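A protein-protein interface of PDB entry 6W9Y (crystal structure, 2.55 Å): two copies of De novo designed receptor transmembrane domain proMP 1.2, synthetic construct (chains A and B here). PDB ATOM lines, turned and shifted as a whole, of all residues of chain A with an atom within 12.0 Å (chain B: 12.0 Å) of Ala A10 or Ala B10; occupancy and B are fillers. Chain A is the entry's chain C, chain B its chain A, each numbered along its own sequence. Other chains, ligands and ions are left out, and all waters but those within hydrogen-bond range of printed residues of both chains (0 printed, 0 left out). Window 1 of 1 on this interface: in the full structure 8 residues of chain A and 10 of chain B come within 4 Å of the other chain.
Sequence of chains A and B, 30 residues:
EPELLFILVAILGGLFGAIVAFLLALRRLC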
ATOM      1  N   PRO A   2      -6.087 -27.297  27.177  1.00  0.00           N
ATOM      2  CA  PRO A   2      -6.941 -26.144  26.876  1.00  0.00           C
ATOM      3  C   PRO A   2      -7.964 -26.448  25.787  1.00  0.00           C
ATOM      4  O   PRO A   2      -7.846 -25.946  24.670  1.00  0.00           O
ATOM      5  CB  PRO A   2      -5.945 -25.083  26.408  1.00  0.00           C
ATOM      6  CG  PRO A   2      -4.804 -25.866  25.856  1.00  0.00           C
ATOM      7  CD  PRO A   2      -4.704 -27.098  26.708  1.00  0.00           C
ATOM      8  N   GLU A   3      -8.962 -27.268  26.122  1.00  0.00           N
ATOM      9  CA  GLU A   3      -9.988 -27.643  25.155  1.00  0.00           C
ATOM     10  C   GLU A   3     -10.904 -26.476  24.805  1.00  0.00           C
ATOM     11  O   GLU A   3     -11.627 -26.546  23.806  1.00  0.00           O
ATOM     12  CB  GLU A   3     -10.806 -28.818  25.699  1.00  0.00           C
ATOM     13  CG  GLU A   3     -11.612 -29.570  24.652  1.00  0.00           C
ATOM     14  CD  GLU A   3     -12.280 -30.808  25.218  1.00  0.00           C
ATOM     15  OE1 GLU A   3     -12.073 -31.104  26.414  1.00  0.00           O
ATOM     16  OE2 GLU A   3     -13.012 -31.485  24.465  1.00  0.00           O
ATOM     17  N   LEU A   4     -10.879 -25.401  25.596  1.00  0.00           N
ATOM     18  CA  LEU A   4     -11.750 -24.259  25.332  1.00  0.00           C
ATOM     19  C   LEU A   4     -11.281 -23.473  24.113  1.00  0.00           C
ATOM     20  O   LEU A   4     -12.080 -23.153  23.223  1.00  0.00           O
ATOM     21  CB  LEU A   4     -11.811 -23.355  26.563  1.00  0.00           C
ATOM     22  CG  LEU A   4     -12.547 -22.023  26.402  1.00  0.00           C
ATOM     23  CD1 LEU A   4     -13.999 -22.262  26.025  1.00  0.00           C
ATOM     24  CD2 LEU A   4     -12.445 -21.198  27.674  1.00  0.00           C
ATOM     25  N   LEU A   5      -9.989 -23.146  24.054  1.00  0.00           N
ATOM     26  CA  LEU A   5      -9.475 -22.330  22.962  1.00  0.00           C
ATOM     27  C   LEU A   5      -9.286 -23.114  21.671  1.00  0.00           C
ATOM     28  O   LEU A   5      -9.204 -22.500  20.602  1.00  0.00           O
ATOM     29  CB  LEU A   5      -8.153 -21.668  23.365  1.00  0.00           C
ATOM     30  CG  LEU A   5      -8.256 -20.243  23.921  1.00  0.00           C
ATOM     31  CD1 LEU A   5      -9.077 -20.203  25.203  1.00  0.00           C
ATOM     32  CD2 LEU A   5      -6.873 -19.649  24.150  1.00  0.00           C
ATOM     33  N   PHE A   6      -9.209 -24.445  21.736  1.00  0.00           N
ATOM     34  CA  PHE A   6      -9.185 -25.235  20.508  1.00  0.00           C
ATOM     35  C   PHE A   6     -10.479 -25.061  19.724  1.00  0.00           C
ATOM     36  O   PHE A   6     -10.465 -25.018  18.488  1.00  0.00           O
ATOM     37  CB  PHE A   6      -8.948 -26.711  20.831  1.00  0.00           C
ATOM     38  CG  PHE A   6      -7.503 -27.067  21.040  1.00  0.00           C
ATOM     39  CD1 PHE A   6      -6.495 -26.310  20.465  1.00  0.00           C
ATOM     40  CD2 PHE A   6      -7.152 -28.167  21.805  1.00  0.00           C
ATOM     41  CE1 PHE A   6      -5.165 -26.640  20.654  1.00  0.00           C
ATOM     42  CE2 PHE A   6      -5.825 -28.502  21.999  1.00  0.00           C
ATOM     43  CZ  PHE A   6      -4.830 -27.739  21.422  1.00  0.00           C
ATOM     44  N   ILE A   7     -11.608 -24.949  20.427  1.00  0.00           N
ATOM     45  CA  ILE A   7     -12.897 -24.788  19.761  1.00  0.00           C
ATOM     46  C   ILE A   7     -13.042 -23.377  19.205  1.00  0.00           C
ATOM     47  O   ILE A   7     -13.644 -23.172  18.144  1.00  0.00           O
ATOM     48  CB  ILE A   7     -14.038 -25.135  20.733  1.00  0.00           C
ATOM     49  CG1 ILE A   7     -13.864 -26.555  21.275  1.00  0.00           C
ATOM     50  CG2 ILE A   7     -15.393 -24.981  20.057  1.00  0.00           C
ATOM     51  CD1 ILE A   7     -14.906 -26.945  22.298  1.00  0.00           C
ATOM     52  N   LEU A   8     -12.492 -22.384  19.906  1.00  0.00           N
ATOM     53  CA  LEU A   8     -12.601 -21.002  19.446  1.00  0.00           C
ATOM     54  C   LEU A   8     -11.849 -20.796  18.138  1.00  0.00           C
ATOM     55  O   LEU A   8     -12.361 -20.164  17.207  1.00  0.00           O
ATOM     56  CB  LEU A   8     -12.077 -20.054  20.522  1.00  0.00           C
ATOM     57  CG  LEU A   8     -12.811 -20.123  21.859  1.00  0.00           C
ATOM     58  CD1 LEU A   8     -12.037 -19.362  22.917  1.00  0.00           C
ATOM     59  CD2 LEU A   8     -14.221 -19.572  21.713  1.00  0.00           C
ATOM     60  N   VAL A   9     -10.623 -21.315  18.054  1.00  0.00           N
ATOM     61  CA  VAL A   9      -9.860 -21.215  16.814  1.00  0.00           C
ATOM     62  C   VAL A   9     -10.527 -22.023  15.709  1.00  0.00           C
ATOM     63  O   VAL A   9     -10.421 -21.677  14.526  1.00  0.00           O
ATOM     64  CB  VAL A   9      -8.404 -21.656  17.060  1.00  0.00           C
ATOM     65  CG1 VAL A   9      -7.545 -21.418  15.821  1.00  0.00           C
ATOM     66  CG2 VAL A   9      -7.828 -20.923  18.268  1.00  0.00           C
ATOM     67  N   ALA A  10     -11.233 -23.099  16.067  1.00  0.00           N
ATOM     68  CA  ALA A  10     -12.022 -23.826  15.080  1.00  0.00           C
ATOM     69  C   ALA A  10     -13.156 -22.961  14.542  1.00  0.00           C
ATOM     70  O   ALA A  10     -13.465 -23.008  13.346  1.00  0.00           O
ATOM     71  CB  ALA A  10     -12.571 -25.113  15.690  1.00  0.00           C
ATOM     72  N   ILE A  11     -13.791 -22.173  15.412  1.00  0.00           N
ATOM     73  CA  ILE A  11     -14.804 -21.229  14.950  1.00  0.00           C
ATOM     74  C   ILE A  11     -14.162 -20.140  14.101  1.00  0.00           C
ATOM     75  O   ILE A  11     -14.683 -19.771  13.042  1.00  0.00           O
ATOM     76  CB  ILE A  11     -15.569 -20.635  16.147  1.00  0.00           C
ATOM     77  CG1 ILE A  11     -16.293 -21.734  16.927  1.00  0.00           C
ATOM     78  CG2 ILE A  11     -16.556 -19.576  15.681  1.00  0.00           C
ATOM     79  CD1 ILE A  11     -16.975 -21.239  18.185  1.00  0.00           C
ATOM     80  N   LEU A  12     -13.018 -19.616  14.548  1.00  0.00           N
ATOM     81  CA  LEU A  12     -12.307 -18.611  13.764  1.00  0.00           C
ATOM     82  C   LEU A  12     -11.839 -19.184  12.433  1.00  0.00           C
ATOM     83  O   LEU A  12     -11.945 -18.526  11.391  1.00  0.00           O
ATOM     84  CB  LEU A  12     -11.119 -18.068  14.560  1.00  0.00           C
ATOM     85  CG  LEU A  12     -11.441 -17.275  15.826  1.00  0.00           C
ATOM     86  CD1 LEU A  12     -10.162 -16.910  16.563  1.00  0.00           C
ATOM     87  CD2 LEU A  12     -12.244 -16.026  15.487  1.00  0.00           C
ATOM     88  N   GLY A  13     -11.318 -20.413  12.448  1.00  0.00           N
ATOM     89  CA  GLY A  13     -10.910 -21.045  11.204  1.00  0.00           C
ATOM     90  C   GLY A  13     -12.083 -21.338  10.287  1.00  0.00           C
ATOM     91  O   GLY A  13     -11.979 -21.199   9.065  1.00  0.00           O
ATOM     92  N   GLY A  14     -13.215 -21.747  10.862  1.00  0.00           N
ATOM     93  CA  GLY A  14     -14.397 -21.990  10.051  1.00  0.00           C
ATOM     94  C   GLY A  14     -14.948 -20.718   9.438  1.00  0.00           C
ATOM     95  O   GLY A  14     -15.311 -20.691   8.258  1.00  0.00           O
ATOM     96  N   LEU A  15     -15.025 -19.646  10.232  1.00  0.00           N
ATOM     97  CA  LEU A  15     -15.444 -18.358   9.691  1.00  0.00           C
ATOM     98  C   LEU A  15     -14.471 -17.875   8.623  1.00  0.00           C
ATOM     99  O   LEU A  15     -14.881 -17.288   7.614  1.00  0.00           O
ATOM    100  CB  LEU A  15     -15.564 -17.327  10.813  1.00  0.00           C
ATOM    101  CG  LEU A  15     -16.672 -17.539  11.847  1.00  0.00           C
ATOM    102  CD1 LEU A  15     -16.548 -16.523  12.974  1.00  0.00           C
ATOM    103  CD2 LEU A  15     -18.045 -17.456  11.192  1.00  0.00           C
ATOM    104  N   PHE A  16     -13.175 -18.119   8.828  1.00  0.00           N
ATOM    105  CA  PHE A  16     -12.185 -17.790   7.808  1.00  0.00           C
ATOM    106  C   PHE A  16     -12.467 -18.539   6.513  1.00  0.00           C
ATOM    107  O   PHE A  16     -12.362 -17.968   5.421  1.00  0.00           O
ATOM    108  CB  PHE A  16     -10.781 -18.113   8.324  1.00  0.00           C
ATOM    109  CG  PHE A  16      -9.675 -17.685   7.400  1.00  0.00           C
ATOM    110  CD1 PHE A  16      -9.059 -16.456   7.562  1.00  0.00           C
ATOM    111  CD2 PHE A  16      -9.239 -18.518   6.381  1.00  0.00           C
ATOM    112  CE1 PHE A  16      -8.038 -16.060   6.719  1.00  0.00           C
ATOM    113  CE2 PHE A  16      -8.220 -18.128   5.534  1.00  0.00           C
ATOM    114  CZ  PHE A  16      -7.618 -16.896   5.704  1.00  0.00           C
ATOM    115  N   GLY A  17     -12.834 -19.817   6.614  1.00  0.00           N
ATOM    116  CA  GLY A  17     -13.103 -20.597   5.418  1.00  0.00           C
ATOM    117  C   GLY A  17     -14.354 -20.144   4.688  1.00  0.00           C
ATOM    118  O   GLY A  17     -14.407 -20.170   3.456  1.00  0.00           O
ATOM    119  N   ALA A  18     -15.378 -19.725   5.437  1.00  0.00           N
ATOM    120  CA  ALA A  18     -16.605 -19.251   4.807  1.00  0.00           C
ATOM    121  C   ALA A  18     -16.378 -17.934   4.077  1.00  0.00           C
ATOM    122  O   ALA A  18     -16.896 -17.732   2.971  1.00  0.00           O
ATOM    123  CB  ALA A  18     -17.711 -19.102   5.851  1.00  0.00           C
ATOM    124  N   ILE A  19     -15.609 -17.024   4.679  1.00  0.00           N
ATOM    125  CA  ILE A  19     -15.304 -15.761   4.015  1.00  0.00           C
ATOM    126  C   ILE A  19     -14.418 -15.997   2.799  1.00  0.00           C
ATOM    127  O   ILE A  19     -14.493 -15.253   1.813  1.00  0.00           O
ATOM    128  CB  ILE A  19     -14.664 -14.779   5.016  1.00  0.00           C
ATOM    129  CG1 ILE A  19     -15.612 -14.529   6.191  1.00  0.00           C
ATOM    130  CG2 ILE A  19     -14.312 -13.463   4.340  1.00  0.00           C
ATOM    131  CD1 ILE A  19     -16.976 -14.019   5.777  1.00  0.00           C
ATOM    132  N   VAL A  20     -13.578 -17.033   2.836  1.00  0.00           N
ATOM    133  CA  VAL A  20     -12.776 -17.384   1.666  1.00  0.00           C
ATOM    134  C   VAL A  20     -13.681 -17.788   0.508  1.00  0.00           C
ATOM    135  O   VAL A  20     -13.551 -17.280  -0.612  1.00  0.00           O
ATOM    136  CB  VAL A  20     -11.772 -18.498   2.013  1.00  0.00           C
ATOM    137  CG1 VAL A  20     -11.275 -19.182   0.746  1.00  0.00           C
ATOM    138  CG2 VAL A  20     -10.601 -17.928   2.798  1.00  0.00           C
ATOM    139  N   ALA A  21     -14.621 -18.701   0.765  1.00  0.00           N
ATOM    140  CA  ALA A  21     -15.501 -19.181  -0.296  1.00  0.00           C
ATOM    141  C   ALA A  21     -16.412 -18.074  -0.811  1.00  0.00           C
ATOM    142  O   ALA A  21     -16.669 -17.987  -2.017  1.00  0.00           O
ATOM    143  CB  ALA A  21     -16.332 -20.362   0.203  1.00  0.00           C
ATOM    144  N   PRO B   2     -12.784 -35.084  21.263  1.00  0.00           N
ATOM    145  CA  PRO B   2     -12.476 -33.668  21.040  1.00  0.00           C
ATOM    146  C   PRO B   2     -12.173 -33.355  19.577  1.00  0.00           C
ATOM    147  O   PRO B   2     -12.409 -32.231  19.133  1.00  0.00           O
ATOM    148  CB  PRO B   2     -11.242 -33.436  21.916  1.00  0.00           C
ATOM    149  CG  PRO B   2     -10.599 -34.771  22.015  1.00  0.00           C
ATOM    150  CD  PRO B   2     -11.714 -35.775  22.003  1.00  0.00           C
ATOM    151  N   GLU B   3     -11.652 -34.336  18.837  1.00  0.00           N
ATOM    152  CA  GLU B   3     -11.374 -34.112  17.422  1.00  0.00           C
ATOM    153  C   GLU B   3     -12.664 -33.961  16.627  1.00  0.00           C
ATOM    154  O   GLU B   3     -12.744 -33.129  15.717  1.00  0.00           O
ATOM    155  CB  GLU B   3     -10.524 -35.251  16.858  1.00  0.00           C
ATOM    156  CG  GLU B   3      -9.153 -35.400  17.504  1.00  0.00           C
ATOM    157  CD  GLU B   3      -9.212 -36.141  18.825  1.00  0.00           C
ATOM    158  OE1 GLU B   3      -8.483 -35.756  19.763  1.00  0.00           O
ATOM    159  OE2 GLU B   3      -9.999 -37.104  18.926  1.00  0.00           O
ATOM    160  N   LEU B   4     -13.687 -34.750  16.962  1.00  0.00           N
ATOM    161  CA  LEU B   4     -14.957 -34.655  16.250  1.00  0.00           C
ATOM    162  C   LEU B   4     -15.626 -33.307  16.491  1.00  0.00           C
ATOM    163  O   LEU B   4     -16.231 -32.738  15.575  1.00  0.00           O
ATOM    164  CB  LEU B   4     -15.882 -35.799  16.669  1.00  0.00           C
ATOM    165  CG  LEU B   4     -15.315 -37.219  16.547  1.00  0.00           C
ATOM    166  CD1 LEU B   4     -16.348 -38.251  16.976  1.00  0.00           C
ATOM    167  CD2 LEU B   4     -14.820 -37.500  15.132  1.00  0.00           C
ATOM    168  N   LEU B   5     -15.525 -32.775  17.713  1.00  0.00           N
ATOM    169  CA  LEU B   5     -16.133 -31.480  17.999  1.00  0.00           C
ATOM    170  C   LEU B   5     -15.367 -30.341  17.335  1.00  0.00           C
ATOM    171  O   LEU B   5     -15.968 -29.325  16.969  1.00  0.00           O
ATOM    172  CB  LEU B   5     -16.217 -31.258  19.511  1.00  0.00           C
ATOM    173  CG  LEU B   5     -16.918 -29.982  19.995  1.00  0.00           C
ATOM    174  CD1 LEU B   5     -18.326 -29.861  19.417  1.00  0.00           C
ATOM    175  CD2 LEU B   5     -16.960 -29.930  21.514  1.00  0.00           C
ATOM    176  N   PHE B   6     -14.052 -30.494  17.164  1.00  0.00           N
ATOM    177  CA  PHE B   6     -13.258 -29.460  16.507  1.00  0.00           C
ATOM    178  C   PHE B   6     -13.696 -29.270  15.060  1.00  0.00           C
ATOM    179  O   PHE B   6     -13.947 -28.144  14.615  1.00  0.00           O
ATOM    180  CB  PHE B   6     -11.773 -29.820  16.580  1.00  0.00           C
ATOM    181  CG  PHE B   6     -10.868 -28.832  15.895  1.00  0.00           C
ATOM    182  CD1 PHE B   6     -10.510 -29.002  14.566  1.00  0.00           C
ATOM    183  CD2 PHE B   6     -10.367 -27.741  16.583  1.00  0.00           C
ATOM    184  CE1 PHE B   6      -9.678 -28.098  13.937  1.00  0.00           C
ATOM    185  CE2 PHE B   6      -9.533 -26.833  15.959  1.00  0.00           C
ATOM    186  CZ  PHE B   6      -9.188 -27.011  14.634  1.00  0.00           C
ATOM    187  N   ILE B   7     -13.788 -30.368  14.306  1.00  0.00           N
ATOM    188  CA  ILE B   7     -14.190 -30.274  12.907  1.00  0.00           C
ATOM    189  C   ILE B   7     -15.671 -29.936  12.790  1.00  0.00           C
ATOM    190  O   ILE B   7     -16.106 -29.359  11.787  1.00  0.00           O
ATOM    191  CB  ILE B   7     -13.838 -31.582  12.169  1.00  0.00           C
ATOM    192  CG1 ILE B   7     -14.033 -31.426  10.658  1.00  0.00           C
ATOM    193  CG2 ILE B   7     -14.667 -32.742  12.701  1.00  0.00           C
ATOM    194  CD1 ILE B   7     -13.139 -30.376  10.031  1.00  0.00           C
ATOM    195  N   LEU B   8     -16.467 -30.270  13.809  1.00  0.00           N
ATOM    196  CA  LEU B   8     -17.893 -29.962  13.770  1.00  0.00           C
ATOM    197  C   LEU B   8     -18.130 -28.458  13.826  1.00  0.00           C
ATOM    198  O   LEU B   8     -18.761 -27.880  12.933  1.00  0.00           O
ATOM    199  CB  LEU B   8     -18.615 -30.662  14.923  1.00  0.00           C
ATOM    200  CG  LEU B   8     -20.078 -30.265  15.133  1.00  0.00           C
ATOM    201  CD1 LEU B   8     -20.921 -30.650  13.928  1.00  0.00           C
ATOM    202  CD2 LEU B   8     -20.632 -30.891  16.405  1.00  0.00           C
ATOM    203  N   VAL B   9     -17.625 -27.802  14.875  1.00  0.00           N
ATOM    204  CA  VAL B   9     -17.809 -26.363  15.010  1.00  0.00           C
ATOM    205  C   VAL B   9     -17.066 -25.595  13.925  1.00  0.00           C
ATOM    206  O   VAL B   9     -17.399 -24.435  13.655  1.00  0.00           O
ATOM    207  CB  VAL B   9     -17.369 -25.891  16.409  1.00  0.00           C
ATOM    208  CG1 VAL B   9     -18.172 -26.606  17.484  1.00  0.00           C
ATOM    209  CG2 VAL B   9     -15.887 -26.124  16.603  1.00  0.00           C
ATOM    210  N   ALA B  10     -16.060 -26.209  13.297  1.00  0.00           N
ATOM    211  CA  ALA B  10     -15.434 -25.584  12.137  1.00  0.00           C
ATOM    212  C   ALA B  10     -16.378 -25.591  10.943  1.00  0.00           C
ATOM    213  O   ALA B  10     -16.455 -24.607  10.198  1.00  0.00           O
ATOM    214  CB  ALA B  10     -14.126 -26.295  11.793  1.00  0.00           C
ATOM    215  N   ILE B  11     -17.105 -26.693  10.749  1.00  0.00           N
ATOM    216  CA  ILE B  11     -18.112 -26.749   9.695  1.00  0.00           C
ATOM    217  C   ILE B  11     -19.296 -25.857  10.046  1.00  0.00           C
ATOM    218  O   ILE B  11     -19.828 -25.142   9.189  1.00  0.00           O
ATOM    219  CB  ILE B  11     -18.548 -28.205   9.451  1.00  0.00           C
ATOM    220  CG1 ILE B  11     -17.379 -29.027   8.910  1.00  0.00           C
ATOM    221  CG2 ILE B  11     -19.732 -28.259   8.495  1.00  0.00           C
ATOM    222  CD1 ILE B  11     -17.695 -30.496   8.732  1.00  0.00           C
ATOM    223  N   LEU B  12     -19.726 -25.883  11.311  1.00  0.00           N
ATOM    224  CA  LEU B  12     -20.818 -25.012  11.732  1.00  0.00           C
ATOM    225  C   LEU B  12     -20.424 -23.545  11.638  1.00  0.00           C
ATOM    226  O   LEU B  12     -21.263 -22.696  11.320  1.00  0.00           O
ATOM    227  CB  LEU B  12     -21.254 -25.363  13.156  1.00  0.00           C
ATOM    228  CG  LEU B  12     -21.834 -26.765  13.357  1.00  0.00           C
ATOM    229  CD1 LEU B  12     -22.241 -26.983  14.809  1.00  0.00           C
ATOM    230  CD2 LEU B  12     -23.012 -27.009  12.423  1.00  0.00           C
ATOM    231  N   GLY B  13     -19.155 -23.226  11.904  1.00  0.00           N
ATOM    232  CA  GLY B  13     -18.698 -21.855  11.735  1.00  0.00           C
ATOM    233  C   GLY B  13     -18.764 -21.398  10.290  1.00  0.00           C
ATOM    234  O   GLY B  13     -19.194 -20.278  10.001  1.00  0.00           O
ATOM    235  N   GLY B  14     -18.338 -22.259   9.366  1.00  0.00           N
ATOM    236  CA  GLY B  14     -18.467 -21.934   7.956  1.00  0.00           C
ATOM    237  C   GLY B  14     -19.911 -21.925   7.497  1.00  0.00           C
ATOM    238  O   GLY B  14     -20.297 -21.120   6.645  1.00  0.00           O
ATOM    239  N   LEU B  15     -20.729 -22.827   8.048  1.00  0.00           N
ATOM    240  CA  LEU B  15     -22.156 -22.822   7.746  1.00  0.00           C
ATOM    241  C   LEU B  15     -22.821 -21.556   8.273  1.00  0.00           C
ATOM    242  O   LEU B  15     -23.681 -20.970   7.604  1.00  0.00           O
ATOM    243  CB  LEU B  15     -22.815 -24.064   8.347  1.00  0.00           C
ATOM    244  CG  LEU B  15     -24.310 -24.274   8.104  1.00  0.00           C
ATOM    245  CD1 LEU B  15     -24.562 -24.748   6.684  1.00  0.00           C
ATOM    246  CD2 LEU B  15     -24.884 -25.258   9.112  1.00  0.00           C
ATOM    247  N   PHE B  16     -22.427 -21.118   9.469  1.00  0.00           N
ATOM    248  CA  PHE B  16     -22.995 -19.906  10.051  1.00  0.00           C
ATOM    249  C   PHE B  16     -22.455 -18.655   9.368  1.00  0.00           C
ATOM    250  O   PHE B  16     -23.188 -17.678   9.182  1.00  0.00           O
ATOM    251  CB  PHE B  16     -22.708 -19.877  11.553  1.00  0.00           C
ATOM    252  CG  PHE B  16     -23.005 -18.561  12.211  1.00  0.00           C
ATOM    253  CD1 PHE B  16     -24.301 -18.223  12.562  1.00  0.00           C
ATOM    254  CD2 PHE B  16     -21.984 -17.672  12.499  1.00  0.00           C
ATOM    255  CE1 PHE B  16     -24.575 -17.015  13.174  1.00  0.00           C
ATOM    256  CE2 PHE B  16     -22.250 -16.463  13.112  1.00  0.00           C
ATOM    257  CZ  PHE B  16     -23.547 -16.135  13.450  1.00  0.00           C
ATOM    258  N   GLY B  17     -21.176 -18.669   8.984  1.00  0.00           N
ATOM    259  CA  GLY B  17     -20.590 -17.498   8.354  1.00  0.00           C
ATOM    260  C   GLY B  17     -21.156 -17.208   6.979  1.00  0.00           C
ATOM    261  O   GLY B  17     -21.238 -16.045   6.572  1.00  0.00           O
ATOM    262  N   ALA B  18     -21.557 -18.248   6.246  1.00  0.00           N
ATOM    263  CA  ALA B  18     -22.134 -18.035   4.923  1.00  0.00           C
ATOM    264  C   ALA B  18     -23.519 -17.411   5.007  1.00  0.00           C
ATOM    265  O   ALA B  18     -23.894 -16.615   4.138  1.00  0.00           O
ATOM    266  CB  ALA B  18     -22.194 -19.356   4.157  1.00  0.00           C
ATOM    267  N   ILE B  19     -24.286 -17.747   6.044  1.00  0.00           N
ATOM    268  CA  ILE B  19     -25.624 -17.185   6.187  1.00  0.00           C
ATOM    269  C   ILE B  19     -25.544 -15.712   6.566  1.00  0.00           C
ATOM    270  O   ILE B  19     -26.287 -14.879   6.032  1.00  0.00           O
ATOM    271  CB  ILE B  19     -26.434 -17.992   7.217  1.00  0.00           C
ATOM    272  CG1 ILE B  19     -26.423 -19.481   6.857  1.00  0.00           C
ATOM    273  CG2 ILE B  19     -27.857 -17.477   7.285  1.00  0.00           C
ATOM    274  CD1 ILE B  19     -27.105 -20.359   7.880  1.00  0.00           C
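Of the printed residues of chain B, Glu A3 touches Pro B2 (3.7 Å).
Printed residues of chain B within 4 Å of Phe A6: Phe B6.
Of chain B, only Leu B5 (3.7 Å) and Val B9 (3.7 Å) come within 4 Å of Ile A7.
No residue of chain B comes within 4 Å of Leu A8.
No residue of chain B comes within 4 Å of Val A9.
Of chain B, only Phe B6 (3.5 Å), Val B9 (3.6 Å) and Ala B10 (3.5 Å) come within 4 Å of Ala A10.
No residue of chain B comes within 4 Å of Ile A11.
Leu A12 touches none of the printed residues of chain B.
No residue of chain B comes within 4 Å of Gly A13.
Of the printed residues of chain B, Leu A15 touches Gly B13 (3.3 Å) and Gly B17 (3.8 Å).
Of the printed residues of chain B, Ala A18 touches Gly B14 and Ala B18.
Val A20 touches none of the printed residues of chain B.
Leu B4 touches none of the printed residues of chain A.
No residue of chain A comes within 4 Å of Ile B7.
No residue of chain A comes within 4 Å of Leu B8.
Val B9 touches just these residues of chain A: Ile A7 (3.7 Å) and Ala A10 (3.6 Å).
Of the printed residues of chain A, Ala B10 touches Ala A10 and Gly A14.
Ile B11 touches none of the printed residues of chain A.
Of the printed residues of chain A, Gly B17 touches Leu A15.
Of the printed residues of chain A, Ala B18 touches Ala A18 (3.96 Å).
The nearest printed residue of chain B that does not touch Ala A10 is Leu B5 (5.6 Å).
The nearest residue of chain A that does not touch Ala B10 is Ile A11 (5.0 Å).
Hydrophobic or aromatic side chains of chain A within 4 Å of the printed part of chain B: Ile A7, Ala A10, Leu A15 and Ala A18.
Of the 18 printed residues of chain B, 9 touch a printed residue of chain A.
Among the printed residues, 14 pairs touch across the chains.
Among the printed residues, no Asp or Glu carboxylate lies within 4 Å of a Lys or Arg side-chain nitrogen of the other chain.
Among the printed residues, merely in contact across the chains: Phe A6 with Phe B6, Leu A15 with Gly B13, Gly A14 with Ala B10, Ala A18 with Gly B14, Gly A14 with Gly B14, Ala A10 with Ala B10, Ala A10 with Phe B6, Ala A10 with Val B9, Glu A3 with Pro B2, Ile A7 with Val B9, Ile A7 with Leu B5, Leu A15 with Gly B17, Ala A18 with Ala B18 and Gly A14 with Gly B13.
Glu A3 touches Pro B2, but with the chains exchanged Pro A2 does not touch Glu B3 (10.9 Å).
Ile A7 touches Leu B5, but with the chains exchanged Leu A5 does not touch Ile B7 (11.1 Å).
Ala A10 touches Val B9, but with the chains exchanged Val A9 does not touch Ala B10 (6.5 Å).
Gly A14 touches its own counterpart, Gly B14.
Of the 14 pairs that touch across the chains among the printed residues, 4 have their exchanged pair printed and touching as well.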
